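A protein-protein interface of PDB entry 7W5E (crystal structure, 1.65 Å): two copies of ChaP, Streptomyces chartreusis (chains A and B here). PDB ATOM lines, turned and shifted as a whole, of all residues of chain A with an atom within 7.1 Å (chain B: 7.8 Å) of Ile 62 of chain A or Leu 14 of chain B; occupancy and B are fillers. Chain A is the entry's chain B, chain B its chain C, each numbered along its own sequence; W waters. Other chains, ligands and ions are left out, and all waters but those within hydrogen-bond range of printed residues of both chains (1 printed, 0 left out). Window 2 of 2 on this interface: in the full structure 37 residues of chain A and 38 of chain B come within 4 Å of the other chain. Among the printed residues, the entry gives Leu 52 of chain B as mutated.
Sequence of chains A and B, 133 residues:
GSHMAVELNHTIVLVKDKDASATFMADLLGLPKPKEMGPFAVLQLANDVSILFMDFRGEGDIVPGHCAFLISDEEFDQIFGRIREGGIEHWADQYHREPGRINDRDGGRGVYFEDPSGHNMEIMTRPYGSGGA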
ATOM      1  N   ASP A  61       6.087  -4.467  17.920  1.00  0.00           N
ATOM      2  CA  ASP A  61       7.437  -4.570  17.374  1.00  0.00           C
ATOM      3  C   ASP A  61       8.357  -5.397  18.268  1.00  0.00           C
ATOM      4  O   ASP A  61       8.421  -5.187  19.480  1.00  0.00           O
ATOM      5  CB  ASP A  61       8.036  -3.175  17.183  1.00  0.00           C
ATOM      6  CG  ASP A  61       8.967  -3.094  15.988  1.00  0.00           C
ATOM      7  OD1 ASP A  61       9.333  -4.150  15.430  1.00  0.00           O
ATOM      8  OD2 ASP A  61       9.349  -1.967  15.615  1.00  0.00           O
ATOM      9  N   ILE A  62       9.040  -6.365  17.662  1.00  0.00           N
ATOM     10  CA  ILE A  62       9.989  -7.231  18.349  1.00  0.00           C
ATOM     11  C   ILE A  62      11.360  -7.041  17.708  1.00  0.00           C
ATOM     12  O   ILE A  62      11.467  -6.940  16.479  1.00  0.00           O
ATOM     13  CB  ILE A  62       9.550  -8.711  18.328  1.00  0.00           C
ATOM     14  CG1 ILE A  62      10.582  -9.588  19.041  1.00  0.00           C
ATOM     15  CG2 ILE A  62       9.330  -9.190  16.905  1.00  0.00           C
ATOM     16  CD1 ILE A  62      10.099 -10.997  19.311  1.00  0.00           C
ATOM     17  N   VAL A  63      12.399  -6.949  18.533  1.00  0.00           N
ATOM     18  CA  VAL A  63      13.766  -6.852  18.018  1.00  0.00           C
ATOM     19  C   VAL A  63      14.084  -8.125  17.239  1.00  0.00           C
ATOM     20  O   VAL A  63      13.557  -9.197  17.572  1.00  0.00           O
ATOM     21  CB  VAL A  63      14.780  -6.616  19.152  1.00  0.00           C
ATOM     22  CG1 VAL A  63      14.457  -5.329  19.901  1.00  0.00           C
ATOM     23  CG2 VAL A  63      14.807  -7.805  20.107  1.00  0.00           C
ATOM     24  N   PRO A  64      14.912  -8.064  16.182  1.00  0.00           N
ATOM     25  CA  PRO A  64      15.639  -6.878  15.708  1.00  0.00           C
ATOM     26  C   PRO A  64      14.864  -6.009  14.725  1.00  0.00           C
ATOM     27  O   PRO A  64      15.490  -5.233  14.007  1.00  0.00           O
ATOM     28  CB  PRO A  64      16.861  -7.471  15.003  1.00  0.00           C
ATOM     29  CG  PRO A  64      16.444  -8.822  14.587  1.00  0.00           C
ATOM     30  CD  PRO A  64      15.390  -9.301  15.540  1.00  0.00           C
ATOM     31  N   GLY A  65      13.541  -6.133  14.681  1.00  0.00           N
ATOM     32  CA  GLY A  65      12.764  -5.255  13.829  1.00  0.00           C
ATOM     33  C   GLY A  65      12.950  -3.801  14.216  1.00  0.00           C
ATOM     34  O   GLY A  65      13.157  -3.472  15.388  1.00  0.00           O
ATOM     35  N   HIS A  66      12.911  -2.931  13.209  1.00  0.00           N
ATOM     36  CA  HIS A  66      12.974  -1.489  13.421  1.00  0.00           C
ATOM     37  C   HIS A  66      12.686  -0.769  12.110  1.00  0.00           C
ATOM     38  O   HIS A  66      12.704  -1.370  11.031  1.00  0.00           O
ATOM     39  CB  HIS A  66      14.332  -1.051  13.995  1.00  0.00           C
ATOM     40  CG  HIS A  66      15.507  -1.372  13.122  1.00  0.00           C
ATOM     41  ND1 HIS A  66      16.041  -2.638  13.025  1.00  0.00           N
ATOM     42  CD2 HIS A  66      16.271  -0.582  12.329  1.00  0.00           C
ATOM     43  CE1 HIS A  66      17.075  -2.617  12.203  1.00  0.00           C
ATOM     44  NE2 HIS A  66      17.237  -1.381  11.768  1.00  0.00           N
ATOM     45  N   GLN A  94      20.709  -3.372  16.923  1.00  0.00           N
ATOM     46  CA  GLN A  94      19.302  -3.628  16.621  1.00  0.00           C
ATOM     47  C   GLN A  94      18.664  -4.642  17.565  1.00  0.00           C
ATOM     48  O   GLN A  94      17.432  -4.709  17.636  1.00  0.00           O
ATOM     49  CB  GLN A  94      19.146  -4.138  15.188  1.00  0.00           C
ATOM     50  CG  GLN A  94      19.961  -5.390  14.888  1.00  0.00           C
ATOM     51  CD  GLN A  94      19.822  -5.850  13.449  1.00  0.00           C
ATOM     52  OE1 GLN A  94      19.165  -5.199  12.635  1.00  0.00           O
ATOM     53  NE2 GLN A  94      20.442  -6.979  13.127  1.00  0.00           N
ATOM     54  N   GLY A 118       6.370   1.535  21.992  1.00  0.00           N
ATOM     55  CA  GLY A 118       7.244   0.388  21.873  1.00  0.00           C
ATOM     56  C   GLY A 118       7.681   0.077  20.460  1.00  0.00           C
ATOM     57  O   GLY A 118       8.275  -0.983  20.230  1.00  0.00           O
ATOM     58  N   ASN A 120      10.100   0.141  17.385  1.00  0.00           N
ATOM     59  CA  ASN A 120      11.555   0.200  17.373  1.00  0.00           C
ATOM     60  C   ASN A 120      12.034   1.114  16.255  1.00  0.00           C
ATOM     61  O   ASN A 120      11.604   0.977  15.103  1.00  0.00           O
ATOM     62  CB  ASN A 120      12.154  -1.194  17.189  1.00  0.00           C
ATOM     63  CG  ASN A 120      11.902  -2.086  18.369  1.00  0.00           C
ATOM     64  OD1 ASN A 120      11.878  -1.622  19.506  1.00  0.00           O
ATOM     65  ND2 ASN A 120      11.713  -3.377  18.114  1.00  0.00           N
ATOM     66  N   THR B  11      13.359  -0.580   6.473  1.00  0.00           N
ATOM     67  CA  THR B  11      12.322  -0.955   7.417  1.00  0.00           C
ATOM     68  C   THR B  11      12.192  -2.469   7.398  1.00  0.00           C
ATOM     69  O   THR B  11      12.292  -3.092   6.338  1.00  0.00           O
ATOM     70  CB  THR B  11      10.985  -0.271   7.076  1.00  0.00           C
ATOM     71  OG1 THR B  11      10.015  -0.568   8.088  1.00  0.00           O
ATOM     72  CG2 THR B  11      10.449  -0.715   5.711  1.00  0.00           C
ATOM     73  N   ILE B  12      11.971  -3.049   8.570  1.00  0.00           N
ATOM     74  CA  ILE B  12      11.903  -4.497   8.740  1.00  0.00           C
ATOM     75  C   ILE B  12      10.438  -4.906   8.699  1.00  0.00           C
ATOM     76  O   ILE B  12       9.591  -4.291   9.361  1.00  0.00           O
ATOM     77  CB  ILE B  12      12.570  -4.950  10.052  1.00  0.00           C
ATOM     78  CG1 ILE B  12      14.100  -4.979   9.932  1.00  0.00           C
ATOM     79  CG2 ILE B  12      12.068  -6.337  10.460  1.00  0.00           C
ATOM     80  CD1 ILE B  12      14.758  -3.640   9.706  1.00  0.00           C
ATOM     81  N   VAL B  13      10.139  -5.942   7.922  1.00  0.00           N
ATOM     82  CA  VAL B  13       8.779  -6.421   7.725  1.00  0.00           C
ATOM     83  C   VAL B  13       8.721  -7.861   8.214  1.00  0.00           C
ATOM     84  O   VAL B  13       9.475  -8.715   7.729  1.00  0.00           O
ATOM     85  CB  VAL B  13       8.360  -6.303   6.250  1.00  0.00           C
ATOM     86  CG1 VAL B  13       7.037  -6.988   6.010  1.00  0.00           C
ATOM     87  CG2 VAL B  13       8.289  -4.836   5.851  1.00  0.00           C
ATOM     88  N   LEU B  14       7.825  -8.130   9.164  1.00  0.00           N
ATOM     89  CA  LEU B  14       7.721  -9.439   9.803  1.00  0.00           C
ATOM     90  C   LEU B  14       6.812 -10.349   8.984  1.00  0.00           C
ATOM     91  O   LEU B  14       5.655 -10.005   8.730  1.00  0.00           O
ATOM     92  CB  LEU B  14       7.164  -9.299  11.219  1.00  0.00           C
ATOM     93  CG  LEU B  14       7.934  -8.547  12.302  1.00  0.00           C
ATOM     94  CD1 LEU B  14       7.703  -9.199  13.661  1.00  0.00           C
ATOM     95  CD2 LEU B  14       9.404  -8.460  11.979  1.00  0.00           C
ATOM     96  N   VAL B  15       7.328 -11.516   8.590  1.00  0.00           N
ATOM     97  CA  VAL B  15       6.573 -12.482   7.801  1.00  0.00           C
ATOM     98  C   VAL B  15       6.893 -13.887   8.294  1.00  0.00           C
ATOM     99  O   VAL B  15       7.878 -14.118   8.998  1.00  0.00           O
ATOM    100  CB  VAL B  15       6.857 -12.390   6.283  1.00  0.00           C
ATOM    101  CG1 VAL B  15       6.343 -11.072   5.713  1.00  0.00           C
ATOM    102  CG2 VAL B  15       8.337 -12.566   6.007  1.00  0.00           C
ATOM    103  N   LYS B  16       6.018 -14.828   7.933  1.00  0.00           N
ATOM    104  CA  LYS B  16       6.226 -16.221   8.315  1.00  0.00           C
ATOM    105  C   LYS B  16       7.497 -16.786   7.693  1.00  0.00           C
ATOM    106  O   LYS B  16       8.271 -17.479   8.365  1.00  0.00           O
ATOM    107  CB  LYS B  16       5.012 -17.059   7.909  1.00  0.00           C
ATOM    108  N   ASP B  17       7.741 -16.489   6.414  1.00  0.00           N
ATOM    109  CA  ASP B  17       8.894 -17.026   5.687  1.00  0.00           C
ATOM    110  C   ASP B  17       9.522 -15.885   4.890  1.00  0.00           C
ATOM    111  O   ASP B  17       8.987 -15.470   3.856  1.00  0.00           O
ATOM    112  CB  ASP B  17       8.477 -18.183   4.782  1.00  0.00           C
ATOM    113  CG  ASP B  17       9.631 -18.743   3.969  1.00  0.00           C
ATOM    114  OD1 ASP B  17      10.797 -18.399   4.252  1.00  0.00           O
ATOM    115  OD2 ASP B  17       9.371 -19.547   3.049  1.00  0.00           O
ATOM    116  N   LYS B  18      10.664 -15.389   5.376  1.00  0.00           N
ATOM    117  CA  LYS B  18      11.306 -14.237   4.750  1.00  0.00           C
ATOM    118  C   LYS B  18      11.771 -14.524   3.324  1.00  0.00           C
ATOM    119  O   LYS B  18      11.770 -13.617   2.486  1.00  0.00           O
ATOM    120  CB  LYS B  18      12.467 -13.756   5.626  1.00  0.00           C
ATOM    121  CG  LYS B  18      13.755 -14.559   5.521  1.00  0.00           C
ATOM    122  CD  LYS B  18      14.860 -13.894   6.338  1.00  0.00           C
ATOM    123  CE  LYS B  18      16.226 -14.497   6.046  1.00  0.00           C
ATOM    124  NZ  LYS B  18      16.137 -15.911   5.595  1.00  0.00           N
ATOM    125  N   SER B  21       8.668 -14.591   0.778  1.00  0.00           N
ATOM    126  CA  SER B  21       8.139 -13.246   0.563  1.00  0.00           C
ATOM    127  C   SER B  21       9.047 -12.420  -0.340  1.00  0.00           C
ATOM    128  O   SER B  21       8.581 -11.803  -1.306  1.00  0.00           O
ATOM    129  CB  SER B  21       7.931 -12.549   1.906  1.00  0.00           C
ATOM    130  OG  SER B  21       6.932 -13.210   2.663  1.00  0.00           O
ATOM    131  N   PHE B  40      17.929 -10.976   7.682  1.00  0.00           N
ATOM    132  CA  PHE B  40      16.998 -10.332   6.768  1.00  0.00           C
ATOM    133  C   PHE B  40      17.163 -10.851   5.346  1.00  0.00           C
ATOM    134  O   PHE B  40      18.259 -11.223   4.920  1.00  0.00           O
ATOM    135  CB  PHE B  40      17.189  -8.812   6.751  1.00  0.00           C
ATOM    136  CG  PHE B  40      17.192  -8.188   8.107  1.00  0.00           C
ATOM    137  CD1 PHE B  40      16.127  -8.375   8.970  1.00  0.00           C
ATOM    138  CD2 PHE B  40      18.264  -7.413   8.522  1.00  0.00           C
ATOM    139  CE1 PHE B  40      16.134  -7.801  10.229  1.00  0.00           C
ATOM    140  CE2 PHE B  40      18.276  -6.839   9.777  1.00  0.00           C
ATOM    141  CZ  PHE B  40      17.208  -7.031  10.629  1.00  0.00           C
ATOM    142  N   ILE B  51      13.370  -2.851   1.944  1.00  0.00           N
ATOM    143  CA  ILE B  51      12.537  -3.636   2.842  1.00  0.00           C
ATOM    144  C   ILE B  51      13.352  -4.840   3.281  1.00  0.00           C
ATOM    145  O   ILE B  51      13.941  -5.540   2.448  1.00  0.00           O
ATOM    146  CB  ILE B  51      11.229  -4.077   2.168  1.00  0.00           C
ATOM    147  CG1 ILE B  51      10.292  -2.892   1.972  1.00  0.00           C
ATOM    148  CG2 ILE B  51      10.535  -5.149   3.004  1.00  0.00           C
ATOM    149  CD1 ILE B  51       9.046  -3.253   1.171  1.00  0.00           C
ATOM    150  N   LEU B  52      13.401  -5.071   4.582  1.00  0.00           N
ATOM    151  CA  LEU B  52      14.152  -6.179   5.160  1.00  0.00           C
ATOM    152  C   LEU B  52      13.130  -7.166   5.715  1.00  0.00           C
ATOM    153  O   LEU B  52      12.517  -6.920   6.756  1.00  0.00           O
ATOM    154  CB  LEU B  52      15.110  -5.676   6.238  1.00  0.00           C
ATOM    155  CG  LEU B  52      16.505  -5.155   5.855  1.00  0.00           C
ATOM    156  CD1 LEU B  52      16.497  -4.278   4.611  1.00  0.00           C
ATOM    157  CD2 LEU B  52      17.098  -4.382   7.024  1.00  0.00           C
ATOM    158  N   PHE B  53      12.924  -8.272   5.005  1.00  0.00           N
ATOM    159  CA  PHE B  53      12.002  -9.296   5.475  1.00  0.00           C
ATOM    160  C   PHE B  53      12.673 -10.138   6.549  1.00  0.00           C
ATOM    161  O   PHE B  53      13.833 -10.533   6.409  1.00  0.00           O
ATOM    162  CB  PHE B  53      11.555 -10.188   4.318  1.00  0.00           C
ATOM    163  CG  PHE B  53      10.618  -9.514   3.365  1.00  0.00           C
ATOM    164  CD1 PHE B  53       9.262  -9.457   3.632  1.00  0.00           C
ATOM    165  CD2 PHE B  53      11.096  -8.937   2.199  1.00  0.00           C
ATOM    166  CE1 PHE B  53       8.397  -8.838   2.748  1.00  0.00           C
ATOM    167  CE2 PHE B  53      10.239  -8.317   1.316  1.00  0.00           C
ATOM    168  CZ  PHE B  53       8.891  -8.266   1.588  1.00  0.00           C
ATOM    169  N   MET B  54      11.938 -10.410   7.625  1.00  0.00           N
ATOM    170  CA  MET B  54      12.464 -11.205   8.723  1.00  0.00           C
ATOM    171  C   MET B  54      11.408 -12.197   9.186  1.00  0.00           C
ATOM    172  O   MET B  54      10.227 -11.853   9.288  1.00  0.00           O
ATOM    173  CB  MET B  54      12.924 -10.299   9.869  1.00  0.00           C
ATOM    174  CG  MET B  54      13.601 -11.022  11.005  1.00  0.00           C
ATOM    175  SD  MET B  54      14.126  -9.881  12.290  1.00  0.00           S
ATOM    176  CE  MET B  54      12.575  -9.328  12.965  1.00  0.00           C
ATOM    177  N   ASP B  55      11.838 -13.428   9.459  1.00  0.00           N
ATOM    178  CA  ASP B  55      10.924 -14.472   9.925  1.00  0.00           C
ATOM    179  C   ASP B  55      10.298 -14.121  11.271  1.00  0.00           C
ATOM    180  O   ASP B  55      10.905 -13.433  12.092  1.00  0.00           O
ATOM    181  CB  ASP B  55      11.641 -15.821  10.021  1.00  0.00           C
ATOM    182  CG  ASP B  55      12.092 -16.340   8.670  1.00  0.00           C
ATOM    183  OD1 ASP B  55      13.303 -16.585   8.496  1.00  0.00           O
ATOM    184  OD2 ASP B  55      11.235 -16.497   7.777  1.00  0.00           O
ATOM    185  N   ASP B  61       0.701  -9.748   9.689  1.00  0.00           N
ATOM    186  CA  ASP B  61       0.102  -8.576   9.060  1.00  0.00           C
ATOM    187  C   ASP B  61      -1.423  -8.641   9.103  1.00  0.00           C
ATOM    188  O   ASP B  61      -2.021  -9.649   8.739  1.00  0.00           O
ATOM    189  CB  ASP B  61       0.586  -8.444   7.617  1.00  0.00           C
ATOM    190  CG  ASP B  61       0.460  -7.036   7.090  1.00  0.00           C
ATOM    191  OD1 ASP B  61       0.522  -6.858   5.852  1.00  0.00           O
ATOM    192  OD2 ASP B  61       0.287  -6.109   7.911  1.00  0.00           O
ATOM    193  N   CYS B  67       1.999  -2.995   2.617  1.00  0.00           N
ATOM    194  CA  CYS B  67       3.149  -2.300   2.046  1.00  0.00           C
ATOM    195  C   CYS B  67       2.807  -1.928   0.609  1.00  0.00           C
ATOM    196  O   CYS B  67       2.329  -2.772  -0.149  1.00  0.00           O
ATOM    197  CB  CYS B  67       4.400  -3.182   2.079  1.00  0.00           C
ATOM    198  SG  CYS B  67       5.164  -3.381   3.707  1.00  0.00           S
ATOM    199  N   HIS B 119       1.025 -11.763   3.634  1.00  0.00           N
ATOM    200  CA  HIS B 119       1.386 -10.377   3.889  1.00  0.00           C
ATOM    201  C   HIS B 119       0.736  -9.495   2.831  1.00  0.00           C
ATOM    202  O   HIS B 119       0.703  -9.846   1.648  1.00  0.00           O
ATOM    203  CB  HIS B 119       2.903 -10.186   3.893  1.00  0.00           C
ATOM    204  CG  HIS B 119       3.328  -8.844   4.401  1.00  0.00           C
ATOM    205  ND1 HIS B 119       3.613  -7.786   3.567  1.00  0.00           N
ATOM    206  CD2 HIS B 119       3.486  -8.380   5.662  1.00  0.00           C
ATOM    207  CE1 HIS B 119       3.944  -6.732   4.290  1.00  0.00           C
ATOM    208  NE2 HIS B 119       3.868  -7.064   5.566  1.00  0.00           N
HETATM  209  O   HOH W   1      10.095  -4.064  12.158  1.00  0.00           O
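O of His 66 of chain A sits at hydrogen-bond distance from N of Ile 12 of chain B, 3.1 Å away.
The backbone carbonyl oxygen of Pro 64 of chain A is in hydrogen-bond range of a ring nitrogen (ND1) of His 66 of chain A, 2.8 Å away. ND2 of Asn 120 of chain A sits close to O of Gly 65 of chain A, 3.1 Å away. O of Thr 11 of chain B sits at hydrogen-bond distance from N of Leu 52 of chain B (2.9 Å). The backbone carbonyl oxygen (O) of Val 13 of chain B sits at hydrogen-bond distance from the backbone NH (N) of Met 54 of chain B, 3.0 Å away. The backbone NH (N) of Val 15 of chain B lies within hydrogen-bond range of the backbone carbonyl oxygen (O) of Met 54 of chain B (3.0 Å).
Ile 62 of chain A touches Leu 14 of chain B (CG2 to CD1, 3.6 Å). Met 54 of chain B touches Pro 64 of chain A. Gly 65 of chain A touches Ile 12 of chain B (CA to CG2, 3.6 Å). Gly 65 of chain A touches Met 54 of chain B (N to CE, 3.8 Å). Thr 11 of chain B touches His 66 of chain A. Phe 40 of chain B touches Gln 94 of chain A.
Of chain B, only Leu 14 comes within 4 Å of Ile 62 of chain A. Printed residues of chain B within 4 Å of Pro 64 of chain A: Met 54 (3.4 Å). Of the printed residues of chain A, Thr 11 of chain B touches His 66 (3.7 Å). Printed residues of chain A within 4 Å of Ile 12 of chain B: Gly 65 (3.6 Å) and His 66 (3.1 Å). Leu 14 of chain B touches just one residue of chain A: Ile 62. Of the printed residues of chain A, Met 54 of chain B touches Pro 64 and Gly 65. The nearest residue of chain B that does not touch Ile 62 of chain A is Met 54 of chain B (4.4 Å). The nearest printed residue of chain A that does not touch Phe 40 of chain B is Pro 64 of chain A (4.2 Å).
Hydrophobic or aromatic side chains of chain B that line the printed part of chain A: Ile 12, Leu 14, Phe 40 and Met 54. Printed residues of chain A that touch a printed residue of chain B: Ile 62, Pro 64, Gly 65, His 66 and Gln 94. Hydrophobic or aromatic side chains of chain A that line the printed part of chain B: Ile 62, Pro 64 and His 66.
1 position is printed for both chains. Of the 7 pairs that touch across the chains among the printed residues, none has its exchanged pair printed and touching as well.
Water W1 lies within hydrogen-bond range of O of Ile 12 of chain B (2.9 Å), N of His 66 of chain A (3.2 Å) and OD1 of Asp 61 of chain A (3.4 Å).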
